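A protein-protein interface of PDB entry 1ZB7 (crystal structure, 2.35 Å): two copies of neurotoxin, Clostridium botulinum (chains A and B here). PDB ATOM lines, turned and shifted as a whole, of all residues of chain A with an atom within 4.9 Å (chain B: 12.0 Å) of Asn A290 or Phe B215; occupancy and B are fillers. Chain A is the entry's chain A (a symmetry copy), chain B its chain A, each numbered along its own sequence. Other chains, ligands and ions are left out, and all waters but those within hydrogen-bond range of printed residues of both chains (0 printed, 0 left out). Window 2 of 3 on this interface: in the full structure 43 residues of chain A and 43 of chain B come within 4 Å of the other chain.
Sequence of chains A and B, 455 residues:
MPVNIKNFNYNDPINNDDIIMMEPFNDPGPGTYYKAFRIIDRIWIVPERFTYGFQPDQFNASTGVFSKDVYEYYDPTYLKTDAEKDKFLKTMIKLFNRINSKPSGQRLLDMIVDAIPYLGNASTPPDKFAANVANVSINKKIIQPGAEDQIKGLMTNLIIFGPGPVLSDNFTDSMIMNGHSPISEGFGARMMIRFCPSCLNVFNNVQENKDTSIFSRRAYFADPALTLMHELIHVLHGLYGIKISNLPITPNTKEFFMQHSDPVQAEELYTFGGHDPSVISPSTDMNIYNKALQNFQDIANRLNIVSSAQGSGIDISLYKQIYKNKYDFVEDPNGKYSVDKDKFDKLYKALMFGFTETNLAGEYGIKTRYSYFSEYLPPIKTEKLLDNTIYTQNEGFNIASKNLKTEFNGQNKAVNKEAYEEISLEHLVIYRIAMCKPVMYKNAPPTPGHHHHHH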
ATOM      1  N   LEU A 247     -24.600  13.545 -12.477  1.00  0.00           N
ATOM      2  CA  LEU A 247     -24.775  13.030 -13.844  1.00  0.00           C
ATOM      3  C   LEU A 247     -25.306  11.578 -13.797  1.00  0.00           C
ATOM      4  O   LEU A 247     -24.956  10.818 -12.897  1.00  0.00           O
ATOM      5  CB  LEU A 247     -23.443  13.036 -14.567  1.00  0.00           C
ATOM      6  CG  LEU A 247     -22.857  14.354 -15.011  1.00  0.00           C
ATOM      7  CD1 LEU A 247     -21.314  14.296 -15.207  1.00  0.00           C
ATOM      8  CD2 LEU A 247     -23.524  14.695 -16.347  1.00  0.00           C
ATOM      9  N   SER A 283     -14.218  16.750  -8.794  1.00  0.00           N
ATOM     10  CA  SER A 283     -14.979  16.998  -9.996  1.00  0.00           C
ATOM     11  C   SER A 283     -16.493  16.943  -9.842  1.00  0.00           C
ATOM     12  O   SER A 283     -17.189  17.751 -10.451  1.00  0.00           O
ATOM     13  CB  SER A 283     -14.611  15.990 -11.053  1.00  0.00           C
ATOM     14  OG  SER A 283     -13.330  16.257 -11.525  1.00  0.00           O
ATOM     15  N   MET A 286     -17.564  20.022  -7.919  1.00  0.00           N
ATOM     16  CA  MET A 286     -17.512  21.179  -8.790  1.00  0.00           C
ATOM     17  C   MET A 286     -18.674  21.261  -9.784  1.00  0.00           C
ATOM     18  O   MET A 286     -19.289  22.289  -9.924  1.00  0.00           O
ATOM     19  CB  MET A 286     -16.174  21.251  -9.549  1.00  0.00           C
ATOM     20  CG  MET A 286     -15.846  22.754  -9.986  1.00  0.00           C
ATOM     21  SD  MET A 286     -14.226  22.662 -10.721  1.00  0.00           S
ATOM     22  CE  MET A 286     -13.389  21.286  -9.806  1.00  0.00           C
ATOM     23  N   ASN A 287     -18.955  20.163 -10.466  1.00  0.00           N
ATOM     24  CA  ASN A 287     -20.147  20.013 -11.305  1.00  0.00           C
ATOM     25  C   ASN A 287     -21.475  20.495 -10.595  1.00  0.00           C
ATOM     26  O   ASN A 287     -22.232  21.302 -11.124  1.00  0.00           O
ATOM     27  CB  ASN A 287     -20.216  18.542 -11.721  1.00  0.00           C
ATOM     28  CG  ASN A 287     -21.275  18.257 -12.753  1.00  0.00           C
ATOM     29  OD1 ASN A 287     -21.482  18.995 -13.684  1.00  0.00           O
ATOM     30  ND2 ASN A 287     -21.968  17.155 -12.567  1.00  0.00           N
ATOM     31  N   ILE A 288     -21.725  19.976  -9.401  1.00  0.00           N
ATOM     32  CA  ILE A 288     -22.843  20.400  -8.608  1.00  0.00           C
ATOM     33  C   ILE A 288     -22.766  21.912  -8.187  1.00  0.00           C
ATOM     34  O   ILE A 288     -23.770  22.622  -8.257  1.00  0.00           O
ATOM     35  CB  ILE A 288     -23.064  19.399  -7.392  1.00  0.00           C
ATOM     36  CG1 ILE A 288     -23.525  18.045  -7.995  1.00  0.00           C
ATOM     37  CG2 ILE A 288     -24.123  19.951  -6.468  1.00  0.00           C
ATOM     38  CD1 ILE A 288     -23.667  16.966  -7.075  1.00  0.00           C
ATOM     39  N   TYR A 289     -21.585  22.364  -7.757  1.00  0.00           N
ATOM     40  CA  TYR A 289     -21.326  23.780  -7.547  1.00  0.00           C
ATOM     41  C   TYR A 289     -21.714  24.643  -8.757  1.00  0.00           C
ATOM     42  O   TYR A 289     -22.443  25.632  -8.613  1.00  0.00           O
ATOM     43  CB  TYR A 289     -19.851  24.038  -7.152  1.00  0.00           C
ATOM     44  CG  TYR A 289     -19.505  25.478  -6.800  1.00  0.00           C
ATOM     45  CD1 TYR A 289     -19.539  25.907  -5.472  1.00  0.00           C
ATOM     46  CD2 TYR A 289     -19.128  26.401  -7.783  1.00  0.00           C
ATOM     47  CE1 TYR A 289     -19.193  27.152  -5.145  1.00  0.00           C
ATOM     48  CE2 TYR A 289     -18.791  27.723  -7.448  1.00  0.00           C
ATOM     49  CZ  TYR A 289     -18.821  28.073  -6.136  1.00  0.00           C
ATOM     50  OH  TYR A 289     -18.518  29.370  -5.740  1.00  0.00           O
ATOM     51  N   ASN A 290     -21.259  24.245  -9.931  1.00  0.00           N
ATOM     52  CA  ASN A 290     -21.425  25.030 -11.156  1.00  0.00           C
ATOM     53  C   ASN A 290     -22.875  25.059 -11.611  1.00  0.00           C
ATOM     54  O   ASN A 290     -23.351  26.051 -12.156  1.00  0.00           O
ATOM     55  CB  ASN A 290     -20.548  24.441 -12.311  1.00  0.00           C
ATOM     56  CG  ASN A 290     -19.051  24.838 -12.197  1.00  0.00           C
ATOM     57  OD1 ASN A 290     -18.679  25.636 -11.302  1.00  0.00           O
ATOM     58  ND2 ASN A 290     -18.179  24.235 -13.078  1.00  0.00           N
ATOM     59  N   LYS A 291     -23.550  23.925 -11.466  1.00  0.00           N
ATOM     60  CA  LYS A 291     -24.970  23.841 -11.787  1.00  0.00           C
ATOM     61  C   LYS A 291     -25.855  24.641 -10.781  1.00  0.00           C
ATOM     62  O   LYS A 291     -26.829  25.255 -11.186  1.00  0.00           O
ATOM     63  CB  LYS A 291     -25.400  22.356 -11.945  1.00  0.00           C
ATOM     64  CG  LYS A 291     -26.828  22.075 -12.604  1.00  0.00           C
ATOM     65  CD  LYS A 291     -27.502  23.275 -13.463  1.00  0.00           C
ATOM     66  CE  LYS A 291     -28.553  22.738 -14.464  1.00  0.00           C
ATOM     67  NZ  LYS A 291     -29.052  21.392 -14.031  1.00  0.00           N
ATOM     68  N   ALA A 292     -25.501  24.697  -9.510  1.00  0.00           N
ATOM     69  CA  ALA A 292     -26.215  25.542  -8.590  1.00  0.00           C
ATOM     70  C   ALA A 292     -26.001  27.051  -8.981  1.00  0.00           C
ATOM     71  O   ALA A 292     -26.935  27.858  -8.972  1.00  0.00           O
ATOM     72  CB  ALA A 292     -25.734  25.250  -7.183  1.00  0.00           C
ATOM     73  N   LEU A 293     -24.779  27.397  -9.378  1.00  0.00           N
ATOM     74  CA  LEU A 293     -24.447  28.748  -9.723  1.00  0.00           C
ATOM     75  C   LEU A 293     -25.252  29.178 -10.956  1.00  0.00           C
ATOM     76  O   LEU A 293     -25.937  30.172 -10.908  1.00  0.00           O
ATOM     77  CB  LEU A 293     -22.948  28.899  -9.931  1.00  0.00           C
ATOM     78  CG  LEU A 293     -22.446  30.241 -10.442  1.00  0.00           C
ATOM     79  CD1 LEU A 293     -22.734  31.329  -9.494  1.00  0.00           C
ATOM     80  CD2 LEU A 293     -20.955  30.111 -10.746  1.00  0.00           C
ATOM     81  N   GLN A 294     -25.229  28.361 -11.994  1.00  0.00           N
ATOM     82  CA  GLN A 294     -26.007  28.559 -13.188  1.00  0.00           C
ATOM     83  C   GLN A 294     -27.522  28.664 -12.872  1.00  0.00           C
ATOM     84  O   GLN A 294     -28.209  29.508 -13.418  1.00  0.00           O
ATOM     85  CB  GLN A 294     -25.698  27.433 -14.219  1.00  0.00           C
ATOM     86  CG  GLN A 294     -26.293  27.604 -15.631  1.00  0.00           C
ATOM     87  CD  GLN A 294     -26.004  28.996 -16.262  1.00  0.00           C
ATOM     88  OE1 GLN A 294     -24.902  29.210 -16.778  1.00  0.00           O
ATOM     89  NE2 GLN A 294     -26.989  29.924 -16.250  1.00  0.00           N
ATOM     90  N   ASN B 204     -16.325   4.568 -13.982  1.00  0.00           N
ATOM     91  CA  ASN B 204     -16.497   5.953 -14.358  1.00  0.00           C
ATOM     92  C   ASN B 204     -15.626   6.953 -13.634  1.00  0.00           C
ATOM     93  O   ASN B 204     -15.239   6.736 -12.529  1.00  0.00           O
ATOM     94  CB  ASN B 204     -17.889   6.425 -13.936  1.00  0.00           C
ATOM     95  CG  ASN B 204     -18.909   6.103 -14.915  1.00  0.00           C
ATOM     96  OD1 ASN B 204     -19.857   5.408 -14.583  1.00  0.00           O
ATOM     97  ND2 ASN B 204     -18.743   6.586 -16.145  1.00  0.00           N
ATOM     98  N   ASN B 205     -15.446   8.113 -14.244  1.00  0.00           N
ATOM     99  CA  ASN B 205     -14.915   9.308 -13.631  1.00  0.00           C
ATOM    100  C   ASN B 205     -15.709  10.434 -14.250  1.00  0.00           C
ATOM    101  O   ASN B 205     -15.831  10.528 -15.462  1.00  0.00           O
ATOM    102  CB  ASN B 205     -13.489   9.541 -14.070  1.00  0.00           C
ATOM    103  CG  ASN B 205     -12.450   9.253 -13.002  1.00  0.00           C
ATOM    104  OD1 ASN B 205     -11.430  10.000 -12.959  1.00  0.00           O
ATOM    105  ND2 ASN B 205     -12.639   8.169 -12.171  1.00  0.00           N
ATOM    106  N   VAL B 206     -16.239  11.292 -13.392  1.00  0.00           N
ATOM    107  CA  VAL B 206     -16.772  12.541 -13.776  1.00  0.00           C
ATOM    108  C   VAL B 206     -15.559  13.451 -14.066  1.00  0.00           C
ATOM    109  O   VAL B 206     -14.680  13.671 -13.200  1.00  0.00           O
ATOM    110  CB  VAL B 206     -17.672  13.121 -12.656  1.00  0.00           C
ATOM    111  CG1 VAL B 206     -18.202  14.492 -13.017  1.00  0.00           C
ATOM    112  CG2 VAL B 206     -18.794  12.194 -12.421  1.00  0.00           C
ATOM    113  N   GLN B 207     -15.522  13.963 -15.294  1.00  0.00           N
ATOM    114  CA  GLN B 207     -14.351  14.696 -15.755  1.00  0.00           C
ATOM    115  C   GLN B 207     -14.647  16.004 -16.522  1.00  0.00           C
ATOM    116  O   GLN B 207     -15.643  16.127 -17.284  1.00  0.00           O
ATOM    117  CB  GLN B 207     -13.333  13.759 -16.456  1.00  0.00           C
ATOM    118  CG  GLN B 207     -12.235  13.328 -15.455  1.00  0.00           C
ATOM    119  CD  GLN B 207     -11.498  12.003 -15.786  1.00  0.00           C
ATOM    120  OE1 GLN B 207     -11.720  11.380 -16.839  1.00  0.00           O
ATOM    121  NE2 GLN B 207     -10.631  11.583 -14.872  1.00  0.00           N
ATOM    122  N   GLU B 208     -13.786  16.972 -16.187  1.00  0.00           N
ATOM    123  CA  GLU B 208     -13.766  18.338 -16.743  1.00  0.00           C
ATOM    124  C   GLU B 208     -13.286  18.321 -18.199  1.00  0.00           C
ATOM    125  O   GLU B 208     -12.137  17.895 -18.429  1.00  0.00           O
ATOM    126  CB  GLU B 208     -12.800  19.199 -15.877  1.00  0.00           C
ATOM    127  CG  GLU B 208     -12.869  20.758 -16.026  1.00  0.00           C
ATOM    128  CD  GLU B 208     -14.287  21.330 -15.951  1.00  0.00           C
ATOM    129  OE1 GLU B 208     -15.228  20.626 -16.388  1.00  0.00           O
ATOM    130  OE2 GLU B 208     -14.459  22.487 -15.490  1.00  0.00           O
ATOM    131  N   ASN B 209     -14.159  18.703 -19.151  1.00  0.00           N
ATOM    132  CA  ASN B 209     -13.829  18.701 -20.626  1.00  0.00           C
ATOM    133  C   ASN B 209     -12.500  19.435 -20.923  1.00  0.00           C
ATOM    134  O   ASN B 209     -12.475  20.581 -21.458  1.00  0.00           O
ATOM    135  CB  ASN B 209     -14.968  19.277 -21.522  1.00  0.00           C
ATOM    136  CG  ASN B 209     -15.279  18.396 -22.759  1.00  0.00           C
ATOM    137  OD1 ASN B 209     -15.343  17.157 -22.655  1.00  0.00           O
ATOM    138  ND2 ASN B 209     -15.497  19.045 -23.925  1.00  0.00           N
ATOM    139  N   LYS B 210     -11.417  18.726 -20.571  1.00  0.00           N
ATOM    140  CA  LYS B 210     -10.071  19.278 -20.499  1.00  0.00           C
ATOM    141  C   LYS B 210     -10.124  20.796 -20.203  1.00  0.00           C
ATOM    142  O   LYS B 210     -10.837  21.253 -19.234  1.00  0.00           O
ATOM    143  CB  LYS B 210      -9.315  18.887 -21.778  1.00  0.00           C
ATOM    144  CG  LYS B 210      -9.147  17.326 -21.839  1.00  0.00           C
ATOM    145  CD  LYS B 210      -7.749  16.851 -21.484  1.00  0.00           C
ATOM    146  CE  LYS B 210      -6.731  17.183 -22.601  1.00  0.00           C
ATOM    147  NZ  LYS B 210      -7.333  17.885 -23.794  1.00  0.00           N
ATOM    148  N   ILE B 214     -17.576  21.999 -19.493  1.00  0.00           N
ATOM    149  CA  ILE B 214     -18.619  20.988 -19.312  1.00  0.00           C
ATOM    150  C   ILE B 214     -18.052  19.688 -18.687  1.00  0.00           C
ATOM    151  O   ILE B 214     -16.934  19.276 -18.983  1.00  0.00           O
ATOM    152  CB  ILE B 214     -19.465  20.706 -20.653  1.00  0.00           C
ATOM    153  CG1 ILE B 214     -19.962  19.234 -20.746  1.00  0.00           C
ATOM    154  CG2 ILE B 214     -18.696  21.148 -21.975  1.00  0.00           C
ATOM    155  CD1 ILE B 214     -21.428  19.036 -20.253  1.00  0.00           C
ATOM    156  N   PHE B 215     -18.858  19.096 -17.797  1.00  0.00           N
ATOM    157  CA  PHE B 215     -18.556  17.870 -17.052  1.00  0.00           C
ATOM    158  C   PHE B 215     -19.308  16.706 -17.675  1.00  0.00           C
ATOM    159  O   PHE B 215     -20.480  16.852 -18.083  1.00  0.00           O
ATOM    160  CB  PHE B 215     -18.972  18.011 -15.581  1.00  0.00           C
ATOM    161  CG  PHE B 215     -18.005  18.782 -14.762  1.00  0.00           C
ATOM    162  CD1 PHE B 215     -16.881  18.170 -14.257  1.00  0.00           C
ATOM    163  CD2 PHE B 215     -18.198  20.155 -14.539  1.00  0.00           C
ATOM    164  CE1 PHE B 215     -15.959  18.889 -13.514  1.00  0.00           C
ATOM    165  CE2 PHE B 215     -17.287  20.881 -13.792  1.00  0.00           C
ATOM    166  CZ  PHE B 215     -16.167  20.239 -13.256  1.00  0.00           C
ATOM    167  N   SER B 216     -18.620  15.560 -17.757  1.00  0.00           N
ATOM    168  CA  SER B 216     -19.223  14.357 -18.312  1.00  0.00           C
ATOM    169  C   SER B 216     -18.586  13.113 -17.670  1.00  0.00           C
ATOM    170  O   SER B 216     -17.528  13.189 -17.036  1.00  0.00           O
ATOM    171  CB  SER B 216     -19.076  14.320 -19.848  1.00  0.00           C
ATOM    172  OG  SER B 216     -17.749  13.936 -20.251  1.00  0.00           O
ATOM    173  N   ARG B 217     -19.240  11.974 -17.869  1.00  0.00           N
ATOM    174  CA  ARG B 217     -18.779  10.724 -17.326  1.00  0.00           C
ATOM    175  C   ARG B 217     -17.858  10.068 -18.318  1.00  0.00           C
ATOM    176  O   ARG B 217     -18.242   9.795 -19.438  1.00  0.00           O
ATOM    177  CB  ARG B 217     -19.936   9.803 -17.033  1.00  0.00           C
ATOM    178  CG  ARG B 217     -20.706  10.216 -15.806  1.00  0.00           C
ATOM    179  CD  ARG B 217     -21.287   9.044 -15.147  1.00  0.00           C
ATOM    180  NE  ARG B 217     -22.104   9.467 -14.025  1.00  0.00           N
ATOM    181  CZ  ARG B 217     -21.701   9.449 -12.774  1.00  0.00           C
ATOM    182  NH1 ARG B 217     -20.492   9.000 -12.496  1.00  0.00           N
ATOM    183  NH2 ARG B 217     -22.523   9.868 -11.796  1.00  0.00           N
ATOM    184  N   ARG B 218     -16.629   9.845 -17.900  1.00  0.00           N
ATOM    185  CA  ARG B 218     -15.706   9.121 -18.737  1.00  0.00           C
ATOM    186  C   ARG B 218     -15.467   7.685 -18.213  1.00  0.00           C
ATOM    187  O   ARG B 218     -15.224   7.485 -17.059  1.00  0.00           O
ATOM    188  CB  ARG B 218     -14.432   9.954 -18.902  1.00  0.00           C
ATOM    189  CG  ARG B 218     -13.686   9.705 -20.164  1.00  0.00           C
ATOM    190  CD  ARG B 218     -14.578   9.370 -21.422  1.00  0.00           C
ATOM    191  NE  ARG B 218     -14.861  10.436 -22.396  1.00  0.00           N
ATOM    192  CZ  ARG B 218     -13.919  11.029 -23.131  1.00  0.00           C
ATOM    193  NH1 ARG B 218     -12.625  10.738 -22.938  1.00  0.00           N
ATOM    194  NH2 ARG B 218     -14.278  11.964 -24.036  1.00  0.00           N
ATOM    195  N   ALA B 219     -15.596   6.715 -19.110  1.00  0.00           N
ATOM    196  CA  ALA B 219     -15.511   5.321 -18.846  1.00  0.00           C
ATOM    197  C   ALA B 219     -14.059   4.830 -18.970  1.00  0.00           C
ATOM    198  O   ALA B 219     -13.361   5.127 -19.950  1.00  0.00           O
ATOM    199  CB  ALA B 219     -16.420   4.591 -19.787  1.00  0.00           C
ATOM    200  N   TYR B 220     -13.586   4.059 -17.975  1.00  0.00           N
ATOM    201  CA  TYR B 220     -12.273   3.448 -18.051  1.00  0.00           C
ATOM    202  C   TYR B 220     -12.387   1.968 -17.723  1.00  0.00           C
ATOM    203  O   TYR B 220     -13.356   1.519 -17.078  1.00  0.00           O
ATOM    204  CB  TYR B 220     -11.264   4.059 -17.115  1.00  0.00           C
ATOM    205  CG  TYR B 220     -10.924   5.480 -17.303  1.00  0.00           C
ATOM    206  CD1 TYR B 220      -9.673   5.873 -17.819  1.00  0.00           C
ATOM    207  CD2 TYR B 220     -11.785   6.458 -16.910  1.00  0.00           C
ATOM    208  CE1 TYR B 220      -9.336   7.209 -17.986  1.00  0.00           C
ATOM    209  CE2 TYR B 220     -11.477   7.799 -17.086  1.00  0.00           C
ATOM    210  CZ  TYR B 220     -10.257   8.184 -17.614  1.00  0.00           C
ATOM    211  OH  TYR B 220     -10.011   9.575 -17.782  1.00  0.00           O
ATOM    212  N   LYS B 367      -4.894   3.980 -13.345  1.00  0.00           N
ATOM    213  CA  LYS B 367      -6.201   4.409 -12.940  1.00  0.00           C
ATOM    214  C   LYS B 367      -7.101   3.284 -12.353  1.00  0.00           C
ATOM    215  O   LYS B 367      -7.267   2.224 -12.926  1.00  0.00           O
ATOM    216  CB  LYS B 367      -6.919   5.093 -14.104  1.00  0.00           C
ATOM    217  CG  LYS B 367      -8.018   5.906 -13.538  1.00  0.00           C
ATOM    218  CD  LYS B 367      -8.450   6.970 -14.346  1.00  0.00           C
ATOM    219  CE  LYS B 367      -9.411   7.831 -13.518  1.00  0.00           C
ATOM    220  NZ  LYS B 367      -9.032   9.281 -13.595  1.00  0.00           N
ATOM    221  N   TYR B 370     -12.665   5.533  -8.117  1.00  0.00           N
ATOM    222  CA  TYR B 370     -12.454   6.626  -7.219  1.00  0.00           C
ATOM    223  C   TYR B 370     -12.661   6.172  -5.771  1.00  0.00           C
ATOM    224  O   TYR B 370     -11.943   6.593  -4.846  1.00  0.00           O
ATOM    225  CB  TYR B 370     -13.455   7.758  -7.546  1.00  0.00           C
ATOM    226  CG  TYR B 370     -13.152   8.894  -6.675  1.00  0.00           C
ATOM    227  CD1 TYR B 370     -12.081   9.735  -6.964  1.00  0.00           C
ATOM    228  CD2 TYR B 370     -13.860   9.090  -5.499  1.00  0.00           C
ATOM    229  CE1 TYR B 370     -11.755  10.756  -6.103  1.00  0.00           C
ATOM    230  CE2 TYR B 370     -13.527  10.048  -4.637  1.00  0.00           C
ATOM    231  CZ  TYR B 370     -12.501  10.906  -4.916  1.00  0.00           C
ATOM    232  OH  TYR B 370     -12.229  11.904  -4.001  1.00  0.00           O
ATOM    233  N   GLU B 407      -3.087  11.492 -18.571  1.00  0.00           N
ATOM    234  CA  GLU B 407      -4.488  11.359 -18.087  1.00  0.00           C
ATOM    235  C   GLU B 407      -4.989   9.896 -18.038  1.00  0.00           C
ATOM    236  O   GLU B 407      -6.188   9.653 -18.085  1.00  0.00           O
ATOM    237  CB  GLU B 407      -5.459  12.194 -18.966  1.00  0.00           C
ATOM    238  CG  GLU B 407      -5.565  13.665 -18.629  1.00  0.00           C
ATOM    239  CD  GLU B 407      -6.518  14.388 -19.559  1.00  0.00           C
ATOM    240  OE1 GLU B 407      -6.505  14.102 -20.775  1.00  0.00           O
ATOM    241  OE2 GLU B 407      -7.294  15.253 -19.121  1.00  0.00           O
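The backbone carbonyl oxygen (O) of Val B206 sits close to the side-chain hydroxyl (OG) of Ser A283 (3.4 Å).
O of Leu A247 sits at hydrogen-bond distance from NH2 of Arg B217 (2.8 Å).
The backbone carbonyl oxygen of Ser B216 lies within hydrogen-bond range of the backbone NH of Gln B207, at 2.8 Å.
Among the printed residues, merely in contact across the chains: Asn A287 with Phe B215, Ser A283 with Phe B215, Asn A290 with Phe B215, Leu A247 with Ser B216, Leu A247 with Val B206, Met A286 with Phe B215 and Leu A247 with Phe B215.
Ser A283 touches two residues of chain B.
No residue of chain B comes within 4 Å of Tyr A289.
Of chain B, only Phe B215 (3.5 Å) comes within 4 Å of Asn A290.
No residue of chain B comes within 4 Å of Ala A292.
No residue of chain B comes within 4 Å of Gln A294.
Of the printed residues of chain A, Phe B215 touches Leu A247, Ser A283, Met A286, Asn A287 and Asn A290.
Of the printed residues of chain A, Ser B216 touches Leu A247 (3.7 Å).
Printed residues of chain A within 4 Å of Arg B217: Leu A247.
Arg B218 touches none of the printed residues of chain A.
Tyr B370 touches none of the printed residues of chain A.
The nearest residue of chain B that does not touch Asn A290 is Glu B208 (4.8 Å).
Of the 17 printed residues of chain B, 4 touch a printed residue of chain A.
Hydrophobic or aromatic side chains of chain B that line the printed part of chain A: Val B206 and Phe B215.
Hydrophobic or aromatic side chains of chain A that line the printed part of chain B: Leu A247 and Met A286.
No position is printed for both chains.
Of the 9 pairs that touch across the chains among the printed residues, none has its exchanged pair printed and touching as well.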
